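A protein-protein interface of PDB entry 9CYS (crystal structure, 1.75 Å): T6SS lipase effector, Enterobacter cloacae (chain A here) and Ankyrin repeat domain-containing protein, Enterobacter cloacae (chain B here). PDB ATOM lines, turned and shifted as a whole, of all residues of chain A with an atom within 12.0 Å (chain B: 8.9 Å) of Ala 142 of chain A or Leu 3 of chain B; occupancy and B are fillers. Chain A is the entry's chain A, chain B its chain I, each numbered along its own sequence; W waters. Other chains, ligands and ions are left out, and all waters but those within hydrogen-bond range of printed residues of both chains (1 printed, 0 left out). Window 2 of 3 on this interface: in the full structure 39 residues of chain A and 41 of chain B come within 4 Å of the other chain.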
ATOM      1  N   ASP A 101       5.036 -16.334  21.921  1.00  0.00           N
ATOM      2  CA  ASP A 101       5.422 -15.574  20.740  1.00  0.00           C
ATOM      3  C   ASP A 101       6.381 -14.472  21.182  1.00  0.00           C
ATOM      4  O   ASP A 101       6.828 -14.447  22.333  1.00  0.00           O
ATOM      5  CB  ASP A 101       4.163 -15.033  20.049  1.00  0.00           C
ATOM      6  CG  ASP A 101       4.383 -14.707  18.580  1.00  0.00           C
ATOM      7  OD1 ASP A 101       5.551 -14.577  18.145  1.00  0.00           O
ATOM      8  OD2 ASP A 101       3.366 -14.583  17.862  1.00  0.00           O
ATOM      9  N   GLU A 134      -4.123  -5.797  19.337  1.00  0.00           N
ATOM     10  CA  GLU A 134      -4.900  -6.448  18.293  1.00  0.00           C
ATOM     11  C   GLU A 134      -5.941  -7.348  18.935  1.00  0.00           C
ATOM     12  O   GLU A 134      -5.612  -8.147  19.818  1.00  0.00           O
ATOM     13  CB  GLU A 134      -4.016  -7.281  17.348  1.00  0.00           C
ATOM     14  CG  GLU A 134      -2.761  -6.599  16.818  1.00  0.00           C
ATOM     15  CD  GLU A 134      -2.233  -7.277  15.562  1.00  0.00           C
ATOM     16  OE1 GLU A 134      -3.056  -7.611  14.679  1.00  0.00           O
ATOM     17  OE2 GLU A 134      -1.001  -7.482  15.458  1.00  0.00           O
ATOM     18  N   PHE A 136      -7.530 -10.591  18.805  1.00  0.00           N
ATOM     19  CA  PHE A 136      -6.851 -11.786  18.300  1.00  0.00           C
ATOM     20  C   PHE A 136      -7.411 -12.356  16.995  1.00  0.00           C
ATOM     21  O   PHE A 136      -6.603 -12.781  16.152  1.00  0.00           O
ATOM     22  CB  PHE A 136      -6.847 -12.864  19.395  1.00  0.00           C
ATOM     23  N   PRO A 137      -8.729 -12.416  16.758  1.00  0.00           N
ATOM     24  CA  PRO A 137      -9.210 -13.000  15.491  1.00  0.00           C
ATOM     25  C   PRO A 137      -8.772 -12.255  14.237  1.00  0.00           C
ATOM     26  O   PRO A 137      -8.781 -12.856  13.155  1.00  0.00           O
ATOM     27  CB  PRO A 137     -10.735 -12.967  15.651  1.00  0.00           C
ATOM     28  CG  PRO A 137     -10.943 -13.053  17.120  1.00  0.00           C
ATOM     29  CD  PRO A 137      -9.847 -12.204  17.699  1.00  0.00           C
ATOM     30  N   THR A 138      -8.396 -10.976  14.328  1.00  0.00           N
ATOM     31  CA  THR A 138      -8.037 -10.196  13.149  1.00  0.00           C
ATOM     32  C   THR A 138      -6.532 -10.132  12.907  1.00  0.00           C
ATOM     33  O   THR A 138      -6.080  -9.307  12.107  1.00  0.00           O
ATOM     34  CB  THR A 138      -8.595  -8.770  13.250  1.00  0.00           C
ATOM     35  OG1 THR A 138      -8.430  -8.271  14.584  1.00  0.00           O
ATOM     36  CG2 THR A 138     -10.074  -8.745  12.872  1.00  0.00           C
ATOM     37  N   LYS A 139      -5.745 -10.968  13.581  1.00  0.00           N
ATOM     38  CA  LYS A 139      -4.313 -10.964  13.333  1.00  0.00           C
ATOM     39  C   LYS A 139      -3.996 -11.710  12.040  1.00  0.00           C
ATOM     40  O   LYS A 139      -4.805 -12.492  11.524  1.00  0.00           O
ATOM     41  CB  LYS A 139      -3.550 -11.583  14.505  1.00  0.00           C
ATOM     42  CG  LYS A 139      -3.799 -10.879  15.828  1.00  0.00           C
ATOM     43  CD  LYS A 139      -3.278 -11.693  17.000  1.00  0.00           C
ATOM     44  CE  LYS A 139      -1.769 -11.635  17.063  1.00  0.00           C
ATOM     45  NZ  LYS A 139      -1.269 -11.824  18.448  1.00  0.00           N
ATOM     46  N   ASN A 140      -2.803 -11.446  11.510  1.00  0.00           N
ATOM     47  CA  ASN A 140      -2.353 -12.092  10.280  1.00  0.00           C
ATOM     48  C   ASN A 140      -2.180 -13.585  10.540  1.00  0.00           C
ATOM     49  O   ASN A 140      -1.287 -14.000  11.287  1.00  0.00           O
ATOM     50  CB  ASN A 140      -1.055 -11.458   9.790  1.00  0.00           C
ATOM     51  CG  ASN A 140      -0.654 -11.938   8.399  1.00  0.00           C
ATOM     52  OD1 ASN A 140      -1.333 -12.773   7.799  1.00  0.00           O
ATOM     53  ND2 ASN A 140       0.451 -11.404   7.880  1.00  0.00           N
ATOM     54  N   MET A 141      -3.046 -14.392   9.933  1.00  0.00           N
ATOM     55  CA  MET A 141      -3.038 -15.829  10.153  1.00  0.00           C
ATOM     56  C   MET A 141      -2.106 -16.558   9.192  1.00  0.00           C
ATOM     57  O   MET A 141      -2.049 -17.793   9.218  1.00  0.00           O
ATOM     58  CB  MET A 141      -4.463 -16.375  10.054  1.00  0.00           C
ATOM     59  CG  MET A 141      -5.389 -15.753  11.098  1.00  0.00           C
ATOM     60  SD  MET A 141      -5.110 -16.384  12.766  1.00  0.00           S
ATOM     61  CE  MET A 141      -5.892 -15.126  13.777  1.00  0.00           C
ATOM     62  N   ALA A 142      -1.382 -15.819   8.346  1.00  0.00           N
ATOM     63  CA  ALA A 142      -0.215 -16.361   7.661  1.00  0.00           C
ATOM     64  C   ALA A 142       0.989 -16.488   8.588  1.00  0.00           C
ATOM     65  O   ALA A 142       1.983 -17.111   8.201  1.00  0.00           O
ATOM     66  CB  ALA A 142       0.149 -15.485   6.458  1.00  0.00           C
ATOM     67  N   ASP A 143       0.929 -15.897   9.783  1.00  0.00           N
ATOM     68  CA  ASP A 143       1.933 -16.102  10.821  1.00  0.00           C
ATOM     69  C   ASP A 143       1.535 -17.327  11.635  1.00  0.00           C
ATOM     70  O   ASP A 143       0.481 -17.333  12.279  1.00  0.00           O
ATOM     71  CB  ASP A 143       2.052 -14.859  11.703  1.00  0.00           C
ATOM     72  CG  ASP A 143       2.581 -13.661  10.942  1.00  0.00           C
ATOM     73  OD1 ASP A 143       3.218 -13.870   9.887  1.00  0.00           O
ATOM     74  OD2 ASP A 143       2.348 -12.517  11.381  1.00  0.00           O
ATOM     75  N   TRP A 144       2.378 -18.363  11.604  1.00  0.00           N
ATOM     76  CA  TRP A 144       1.926 -19.680  12.040  1.00  0.00           C
ATOM     77  C   TRP A 144       1.588 -19.710  13.521  1.00  0.00           C
ATOM     78  O   TRP A 144       0.704 -20.465  13.934  1.00  0.00           O
ATOM     79  CB  TRP A 144       2.969 -20.748  11.705  1.00  0.00           C
ATOM     80  CG  TRP A 144       4.302 -20.657  12.405  1.00  0.00           C
ATOM     81  CD1 TRP A 144       5.417 -19.995  11.969  1.00  0.00           C
ATOM     82  CD2 TRP A 144       4.679 -21.310  13.628  1.00  0.00           C
ATOM     83  NE1 TRP A 144       6.457 -20.182  12.851  1.00  0.00           N
ATOM     84  CE2 TRP A 144       6.029 -20.982  13.880  1.00  0.00           C
ATOM     85  CE3 TRP A 144       4.004 -22.130  14.535  1.00  0.00           C
ATOM     86  CZ2 TRP A 144       6.714 -21.437  15.012  1.00  0.00           C
ATOM     87  CZ3 TRP A 144       4.687 -22.587  15.655  1.00  0.00           C
ATOM     88  CH2 TRP A 144       6.024 -22.241  15.883  1.00  0.00           C
ATOM     89  N   ILE A 145       2.257 -18.893  14.331  1.00  0.00           N
ATOM     90  CA  ILE A 145       1.996 -18.927  15.766  1.00  0.00           C
ATOM     91  C   ILE A 145       0.612 -18.363  16.059  1.00  0.00           C
ATOM     92  O   ILE A 145      -0.135 -18.907  16.882  1.00  0.00           O
ATOM     93  CB  ILE A 145       3.091 -18.157  16.515  1.00  0.00           C
ATOM     94  CG1 ILE A 145       4.332 -19.020  16.657  1.00  0.00           C
ATOM     95  CG2 ILE A 145       2.625 -17.846  17.929  1.00  0.00           C
ATOM     96  CD1 ILE A 145       5.568 -18.215  16.928  1.00  0.00           C
ATOM     97  N   ASN A 146       0.232 -17.284  15.362  1.00  0.00           N
ATOM     98  CA  ASN A 146      -1.124 -16.752  15.483  1.00  0.00           C
ATOM     99  C   ASN A 146      -2.149 -17.777  15.033  1.00  0.00           C
ATOM    100  O   ASN A 146      -3.199 -17.943  15.666  1.00  0.00           O
ATOM    101  CB  ASN A 146      -1.281 -15.478  14.648  1.00  0.00           C
ATOM    102  CG  ASN A 146      -0.405 -14.339  15.135  1.00  0.00           C
ATOM    103  OD1 ASN A 146       0.050 -14.330  16.280  1.00  0.00           O
ATOM    104  ND2 ASN A 146      -0.164 -13.366  14.257  1.00  0.00           N
ATOM    105  N   ASN A 147      -1.872 -18.450  13.919  1.00  0.00           N
ATOM    106  CA  ASN A 147      -2.736 -19.528  13.468  1.00  0.00           C
ATOM    107  C   ASN A 147      -2.882 -20.582  14.561  1.00  0.00           C
ATOM    108  O   ASN A 147      -3.994 -21.019  14.877  1.00  0.00           O
ATOM    109  CB  ASN A 147      -2.157 -20.138  12.193  1.00  0.00           C
ATOM    110  CG  ASN A 147      -3.194 -20.846  11.363  1.00  0.00           C
ATOM    111  OD1 ASN A 147      -3.774 -21.849  11.784  1.00  0.00           O
ATOM    112  ND2 ASN A 147      -3.423 -20.340  10.160  1.00  0.00           N
ATOM    113  N   GLY A 148      -1.760 -20.978  15.170  1.00  0.00           N
ATOM    114  CA  GLY A 148      -1.800 -22.016  16.188  1.00  0.00           C
ATOM    115  C   GLY A 148      -2.532 -21.587  17.443  1.00  0.00           C
ATOM    116  O   GLY A 148      -3.334 -22.347  17.991  1.00  0.00           O
ATOM    117  N   ALA A 149      -2.267 -20.371  17.921  1.00  0.00           N
ATOM    118  CA  ALA A 149      -2.983 -19.884  19.098  1.00  0.00           C
ATOM    119  C   ALA A 149      -4.485 -19.853  18.844  1.00  0.00           C
ATOM    120  O   ALA A 149      -5.278 -20.262  19.699  1.00  0.00           O
ATOM    121  CB  ALA A 149      -2.474 -18.498  19.491  1.00  0.00           C
ATOM    122  N   GLN A 150      -4.896 -19.392  17.663  1.00  0.00           N
ATOM    123  CA  GLN A 150      -6.315 -19.389  17.328  1.00  0.00           C
ATOM    124  C   GLN A 150      -6.886 -20.803  17.334  1.00  0.00           C
ATOM    125  O   GLN A 150      -7.923 -21.065  17.957  1.00  0.00           O
ATOM    126  CB  GLN A 150      -6.526 -18.727  15.964  1.00  0.00           C
ATOM    127  N   GLY A 151      -6.217 -21.736  16.652  1.00  0.00           N
ATOM    128  CA  GLY A 151      -6.754 -23.081  16.535  1.00  0.00           C
ATOM    129  C   GLY A 151      -6.757 -23.849  17.843  1.00  0.00           C
ATOM    130  O   GLY A 151      -7.569 -24.756  18.032  1.00  0.00           O
ATOM    131  N   LEU A 152      -5.855 -23.508  18.754  1.00  0.00           N
ATOM    132  CA  LEU A 152      -5.789 -24.168  20.049  1.00  0.00           C
ATOM    133  C   LEU A 152      -6.675 -23.514  21.099  1.00  0.00           C
ATOM    134  O   LEU A 152      -6.714 -23.992  22.236  1.00  0.00           O
ATOM    135  CB  LEU A 152      -4.345 -24.198  20.543  1.00  0.00           C
ATOM    136  CG  LEU A 152      -3.388 -24.977  19.641  1.00  0.00           C
ATOM    137  CD1 LEU A 152      -1.960 -24.842  20.148  1.00  0.00           C
ATOM    138  CD2 LEU A 152      -3.788 -26.424  19.578  1.00  0.00           C
ATOM    139  N   ASP B   2      -3.791 -23.098   5.316  1.00  0.00           N
ATOM    140  CA  ASP B   2      -3.332 -21.801   4.822  1.00  0.00           C
ATOM    141  C   ASP B   2      -1.807 -21.693   4.840  1.00  0.00           C
ATOM    142  O   ASP B   2      -1.244 -20.731   4.319  1.00  0.00           O
ATOM    143  CB  ASP B   2      -3.945 -20.666   5.647  1.00  0.00           C
ATOM    144  N   LEU B   3      -1.142 -22.678   5.440  1.00  0.00           N
ATOM    145  CA  LEU B   3       0.307 -22.679   5.572  1.00  0.00           C
ATOM    146  C   LEU B   3       0.934 -23.640   4.564  1.00  0.00           C
ATOM    147  O   LEU B   3       0.330 -24.644   4.185  1.00  0.00           O
ATOM    148  CB  LEU B   3       0.716 -23.075   6.999  1.00  0.00           C
ATOM    149  CG  LEU B   3       0.152 -22.223   8.142  1.00  0.00           C
ATOM    150  CD1 LEU B   3       0.574 -22.782   9.499  1.00  0.00           C
ATOM    151  CD2 LEU B   3       0.594 -20.774   8.006  1.00  0.00           C
ATOM    152  N   LYS B   4       2.156 -23.328   4.134  1.00  0.00           N
ATOM    153  CA  LYS B   4       2.855 -24.156   3.165  1.00  0.00           C
ATOM    154  C   LYS B   4       4.181 -24.641   3.738  1.00  0.00           C
ATOM    155  O   LYS B   4       4.987 -23.823   4.206  1.00  0.00           O
ATOM    156  CB  LYS B   4       3.098 -23.384   1.849  1.00  0.00           C
ATOM    157  N   PRO B   5       4.456 -25.948   3.698  1.00  0.00           N
ATOM    158  CA  PRO B   5       5.677 -26.459   4.345  1.00  0.00           C
ATOM    159  C   PRO B   5       6.957 -25.956   3.711  1.00  0.00           C
ATOM    160  O   PRO B   5       7.987 -25.892   4.395  1.00  0.00           O
ATOM    161  CB  PRO B   5       5.538 -27.979   4.201  1.00  0.00           C
ATOM    162  CG  PRO B   5       4.613 -28.158   3.037  1.00  0.00           C
ATOM    163  CD  PRO B   5       3.647 -27.024   3.106  1.00  0.00           C
ATOM    164  N   ASP B   6       6.927 -25.607   2.418  1.00  0.00           N
ATOM    165  CA  ASP B   6       8.107 -25.096   1.729  1.00  0.00           C
ATOM    166  C   ASP B   6       8.610 -23.786   2.306  1.00  0.00           C
ATOM    167  O   ASP B   6       9.771 -23.429   2.077  1.00  0.00           O
ATOM    168  CB  ASP B   6       7.786 -24.887   0.246  1.00  0.00           C
ATOM    169  CG  ASP B   6       6.896 -25.961  -0.298  1.00  0.00           C
ATOM    170  OD1 ASP B   6       5.700 -25.983   0.068  1.00  0.00           O
ATOM    171  OD2 ASP B   6       7.393 -26.785  -1.095  1.00  0.00           O
ATOM    172  N   ASN B   7       7.765 -23.048   3.025  1.00  0.00           N
ATOM    173  CA  ASN B   7       8.225 -21.814   3.646  1.00  0.00           C
ATOM    174  C   ASN B   7       9.132 -22.060   4.844  1.00  0.00           C
ATOM    175  O   ASN B   7       9.819 -21.132   5.280  1.00  0.00           O
ATOM    176  CB  ASN B   7       7.026 -20.959   4.054  1.00  0.00           C
ATOM    177  CG  ASN B   7       6.297 -20.375   2.858  1.00  0.00           C
ATOM    178  OD1 ASN B   7       6.905 -20.108   1.822  1.00  0.00           O
ATOM    179  ND2 ASN B   7       4.994 -20.180   2.994  1.00  0.00           N
ATOM    180  N   TYR B   8       9.171 -23.277   5.375  1.00  0.00           N
ATOM    181  CA  TYR B   8       9.971 -23.556   6.554  1.00  0.00           C
ATOM    182  C   TYR B   8      11.042 -24.604   6.331  1.00  0.00           C
ATOM    183  O   TYR B   8      12.087 -24.544   6.985  1.00  0.00           O
ATOM    184  CB  TYR B   8       9.059 -23.999   7.710  1.00  0.00           C
ATOM    185  CG  TYR B   8       7.808 -23.163   7.808  1.00  0.00           C
ATOM    186  CD1 TYR B   8       7.829 -21.904   8.414  1.00  0.00           C
ATOM    187  CD2 TYR B   8       6.610 -23.618   7.298  1.00  0.00           C
ATOM    188  CE1 TYR B   8       6.684 -21.136   8.493  1.00  0.00           C
ATOM    189  CE2 TYR B   8       5.458 -22.859   7.370  1.00  0.00           C
ATOM    190  CZ  TYR B   8       5.502 -21.618   7.968  1.00  0.00           C
ATOM    191  OH  TYR B   8       4.348 -20.868   8.037  1.00  0.00           O
ATOM    192  N   ALA B  17       7.809 -33.064   6.130  1.00  0.00           N
ATOM    193  CA  ALA B  17       6.778 -32.059   6.342  1.00  0.00           C
ATOM    194  C   ALA B  17       5.591 -32.274   5.424  1.00  0.00           C
ATOM    195  O   ALA B  17       4.458 -31.943   5.786  1.00  0.00           O
ATOM    196  CB  ALA B  17       7.349 -30.657   6.143  1.00  0.00           C
ATOM    197  N   GLU B  21       1.824 -32.860   6.395  1.00  0.00           N
ATOM    198  CA  GLU B  21       0.771 -32.050   5.793  1.00  0.00           C
ATOM    199  C   GLU B  21      -0.372 -32.925   5.300  1.00  0.00           C
ATOM    200  O   GLU B  21      -1.545 -32.567   5.448  1.00  0.00           O
ATOM    201  CB  GLU B  21       1.336 -31.204   4.648  1.00  0.00           C
ATOM    202  CG  GLU B  21       0.297 -30.331   3.955  1.00  0.00           C
ATOM    203  CD  GLU B  21       0.880 -29.491   2.832  1.00  0.00           C
ATOM    204  OE1 GLU B  21       1.876 -29.923   2.211  1.00  0.00           O
ATOM    205  OE2 GLU B  21       0.338 -28.396   2.567  1.00  0.00           O
ATOM    206  N   GLU B  43      11.654 -19.433  10.489  1.00  0.00           N
ATOM    207  CA  GLU B  43      10.648 -18.818  11.367  1.00  0.00           C
ATOM    208  C   GLU B  43      10.469 -19.593  12.675  1.00  0.00           C
ATOM    209  O   GLU B  43       9.386 -19.592  13.254  1.00  0.00           O
ATOM    210  CB  GLU B  43       9.296 -18.688  10.669  1.00  0.00           C
ATOM    211  CG  GLU B  43       9.235 -17.599   9.619  1.00  0.00           C
ATOM    212  CD  GLU B  43       7.902 -17.581   8.913  1.00  0.00           C
ATOM    213  OE1 GLU B  43       6.864 -17.600   9.609  1.00  0.00           O
ATOM    214  OE2 GLU B  43       7.890 -17.555   7.659  1.00  0.00           O
ATOM    215  N   MET B  45      10.072 -22.596  13.056  1.00  0.00           N
ATOM    216  CA  MET B  45       9.294 -23.817  12.899  1.00  0.00           C
ATOM    217  C   MET B  45      10.147 -25.061  13.085  1.00  0.00           C
ATOM    218  O   MET B  45      11.270 -25.151  12.589  1.00  0.00           O
ATOM    219  CB  MET B  45       8.590 -23.867  11.537  1.00  0.00           C
ATOM    220  CG  MET B  45       7.711 -25.107  11.487  1.00  0.00           C
ATOM    221  SD  MET B  45       6.042 -24.968  12.048  1.00  0.00           S
ATOM    222  CE  MET B  45       5.458 -23.556  11.149  1.00  0.00           C
ATOM    223  N   PHE B  49       6.299 -28.749  15.845  1.00  0.00           N
ATOM    224  CA  PHE B  49       5.327 -27.660  15.777  1.00  0.00           C
ATOM    225  C   PHE B  49       4.513 -27.743  14.493  1.00  0.00           C
ATOM    226  O   PHE B  49       3.315 -27.426  14.479  1.00  0.00           O
ATOM    227  CB  PHE B  49       6.033 -26.309  15.860  1.00  0.00           C
ATOM    228  CG  PHE B  49       6.141 -25.757  17.260  1.00  0.00           C
ATOM    229  CD1 PHE B  49       4.993 -25.470  17.986  1.00  0.00           C
ATOM    230  CD2 PHE B  49       7.373 -25.520  17.817  1.00  0.00           C
ATOM    231  CE1 PHE B  49       5.086 -24.958  19.271  1.00  0.00           C
ATOM    232  CE2 PHE B  49       7.468 -24.997  19.100  1.00  0.00           C
ATOM    233  CZ  PHE B  49       6.318 -24.721  19.812  1.00  0.00           C
ATOM    234  N   TRP B  50       5.165 -28.134  13.396  1.00  0.00           N
ATOM    235  CA  TRP B  50       4.460 -28.330  12.135  1.00  0.00           C
ATOM    236  C   TRP B  50       3.361 -29.386  12.273  1.00  0.00           C
ATOM    237  O   TRP B  50       2.245 -29.201  11.769  1.00  0.00           O
ATOM    238  CB  TRP B  50       5.476 -28.699  11.041  1.00  0.00           C
ATOM    239  CG  TRP B  50       4.846 -28.928   9.699  1.00  0.00           C
ATOM    240  CD1 TRP B  50       4.772 -30.108   9.014  1.00  0.00           C
ATOM    241  CD2 TRP B  50       4.175 -27.951   8.896  1.00  0.00           C
ATOM    242  NE1 TRP B  50       4.095 -29.922   7.821  1.00  0.00           N
ATOM    243  CE2 TRP B  50       3.723 -28.606   7.727  1.00  0.00           C
ATOM    244  CE3 TRP B  50       3.918 -26.581   9.047  1.00  0.00           C
ATOM    245  CZ2 TRP B  50       3.019 -27.939   6.722  1.00  0.00           C
ATOM    246  CZ3 TRP B  50       3.222 -25.914   8.037  1.00  0.00           C
ATOM    247  CH2 TRP B  50       2.780 -26.598   6.892  1.00  0.00           C
ATOM    248  N   VAL B  52       1.739 -30.106  15.079  1.00  0.00           N
ATOM    249  CA  VAL B  52       0.655 -29.464  15.828  1.00  0.00           C
ATOM    250  C   VAL B  52      -0.187 -28.588  14.898  1.00  0.00           C
ATOM    251  O   VAL B  52      -1.422 -28.648  14.900  1.00  0.00           O
ATOM    252  CB  VAL B  52       1.213 -28.644  17.009  1.00  0.00           C
ATOM    253  CG1 VAL B  52       0.083 -27.902  17.710  1.00  0.00           C
ATOM    254  CG2 VAL B  52       1.941 -29.540  17.994  1.00  0.00           C
ATOM    255  N   MET B  53       0.485 -27.777  14.081  1.00  0.00           N
ATOM    256  CA  MET B  53      -0.173 -26.876  13.140  1.00  0.00           C
ATOM    257  C   MET B  53      -1.056 -27.620  12.148  1.00  0.00           C
ATOM    258  O   MET B  53      -1.975 -27.023  11.579  1.00  0.00           O
ATOM    259  CB  MET B  53       0.901 -26.081  12.390  1.00  0.00           C
ATOM    260  CG  MET B  53       1.394 -24.770  13.020  1.00  0.00           C
ATOM    261  SD  MET B  53       0.331 -24.059  14.289  1.00  0.00           S
ATOM    262  CE  MET B  53      -1.000 -23.479  13.224  1.00  0.00           C
ATOM    263  N   ASN B  54      -0.791 -28.905  11.916  1.00  0.00           N
ATOM    264  CA  ASN B  54      -1.554 -29.712  10.972  1.00  0.00           C
ATOM    265  C   ASN B  54      -2.537 -30.647  11.669  1.00  0.00           C
ATOM    266  O   ASN B  54      -2.985 -31.635  11.069  1.00  0.00           O
ATOM    267  CB  ASN B  54      -0.597 -30.494  10.072  1.00  0.00           C
ATOM    268  CG  ASN B  54      -0.067 -29.650   8.940  1.00  0.00           C
ATOM    269  OD1 ASN B  54      -0.664 -29.593   7.861  1.00  0.00           O
ATOM    270  ND2 ASN B  54       1.038 -28.951   9.186  1.00  0.00           N
ATOM    271  N   ILE B  56      -5.207 -29.084  13.760  1.00  0.00           N
ATOM    272  CA  ILE B  56      -6.142 -28.153  14.374  1.00  0.00           C
ATOM    273  C   ILE B  56      -7.342 -27.944  13.458  1.00  0.00           C
ATOM    274  O   ILE B  56      -7.312 -28.244  12.260  1.00  0.00           O
ATOM    275  CB  ILE B  56      -5.470 -26.807  14.727  1.00  0.00           C
ATOM    276  CG1 ILE B  56      -4.766 -26.208  13.514  1.00  0.00           C
ATOM    277  CG2 ILE B  56      -4.452 -26.987  15.845  1.00  0.00           C
ATOM    278  CD1 ILE B  56      -4.503 -24.721  13.643  1.00  0.00           C
ATOM    279  N   GLN B  59      -8.747 -30.436  10.938  1.00  0.00           N
ATOM    280  CA  GLN B  59      -7.728 -31.471  10.874  1.00  0.00           C
ATOM    281  C   GLN B  59      -7.400 -32.078  12.242  1.00  0.00           C
ATOM    282  O   GLN B  59      -6.463 -32.876  12.344  1.00  0.00           O
ATOM    283  CB  GLN B  59      -6.474 -30.903  10.204  1.00  0.00           C
ATOM    284  CG  GLN B  59      -6.713 -30.679   8.708  1.00  0.00           C
ATOM    285  CD  GLN B  59      -5.472 -30.338   7.918  1.00  0.00           C
ATOM    286  OE1 GLN B  59      -4.454 -29.926   8.471  1.00  0.00           O
ATOM    287  NE2 GLN B  59      -5.554 -30.502   6.601  1.00  0.00           N
HETATM  288  O   HOH W   1       4.158 -18.495   9.098  1.00  0.00           O
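The backbone carbonyl oxygen (O) of Glu 43 of chain B lies within hydrogen-bond range of the indole nitrogen (NE1) of Trp 144 of chain A (3.0 Å). The backbone carbonyl oxygen of Trp 144 of chain A lies close to the side-chain sulfur of Met 53 of chain B (3.6 Å).
Ala 142 of chain A touches just one residue of chain B: Leu 3 (3.9 Å). Leu 3 of chain B touches two residues of chain A. No residue of chain A comes within 4 Å of Asp 2 of chain B. Lys 4 of chain B touches none of the printed residues of chain A. No residue of chain A comes within 4 Å of Pro 5 of chain B. Of chain A, only Trp 144 (3.5 Å), Asn 147 (3.5 Å) and Gly 148 (3.3 Å) come within 4 Å of Met 53 of chain B. Printed residues of chain A within 4 Å of Ile 56 of chain B: Asn 147 and Leu 152. Of the printed residues of chain B, Asn 147 of chain A touches Met 53 and Ile 56. Of the printed residues of chain A, Phe 49 of chain B touches Trp 144 (3.7 Å). Of the printed residues of chain B, Gly 148 of chain A touches Met 53. Phe 136 of chain A touches none of the printed residues of chain B. The nearest residue of chain B that does not touch Ala 142 of chain A is Tyr 8 of chain B (4.4 Å). The nearest residue of chain A that does not touch Leu 3 of chain B is Met 141 of chain A (4.2 Å).
Water W1 lies within hydrogen-bond range of OH of Tyr 8 of chain B, O of Ala 142 of chain A, OE1 of Glu 43 of chain B and N of Trp 144 of chain A.
Ala 142 of chain A touches Leu 3 of chain B (O to CD2, 3.9 Å). Trp 144 of chain A touches Leu 3 of chain B. Tyr 8 of chain B touches Trp 144 of chain A. Met 45 of chain B touches Trp 144 of chain A (CE to CG, 3.4 Å). Phe 49 of chain B touches Trp 144 of chain A (CD1 to CZ3, 3.7 Å). Asn 147 of chain A touches Met 53 of chain B. Ile 56 of chain B touches Asn 147 of chain A. Gly 148 of chain A touches Met 53 of chain B. Leu 152 of chain A touches Ile 56 of chain B.
Printed residues of chain A that touch a printed residue of chain B: Ala 142, Trp 144, Asn 147, Gly 148 and Leu 152. Of the 18 printed residues of chain B, 7 touch a printed residue of chain A. Hydrophobic or aromatic side chains of chain B that line the printed part of chain A: Leu 3, Tyr 8, Met 45, Phe 49, Met 53 and Ile 56. Among the printed residues, no Asp or Glu carboxylate lies within 4 Å of a Lys or Arg side-chain nitrogen of the other chain.
SD of Met 45 of chain B lies within hydrogen-bond range of N of Trp 50 of chain B, at 3.6 Å. OD1 of Asn 140 of chain A sits at hydrogen-bond distance from N of Ala 142 of chain A (3.1 Å). The backbone carbonyl oxygen of Met 141 of chain A sits at hydrogen-bond distance from the side-chain amide nitrogen of Asn 147 of chain A.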
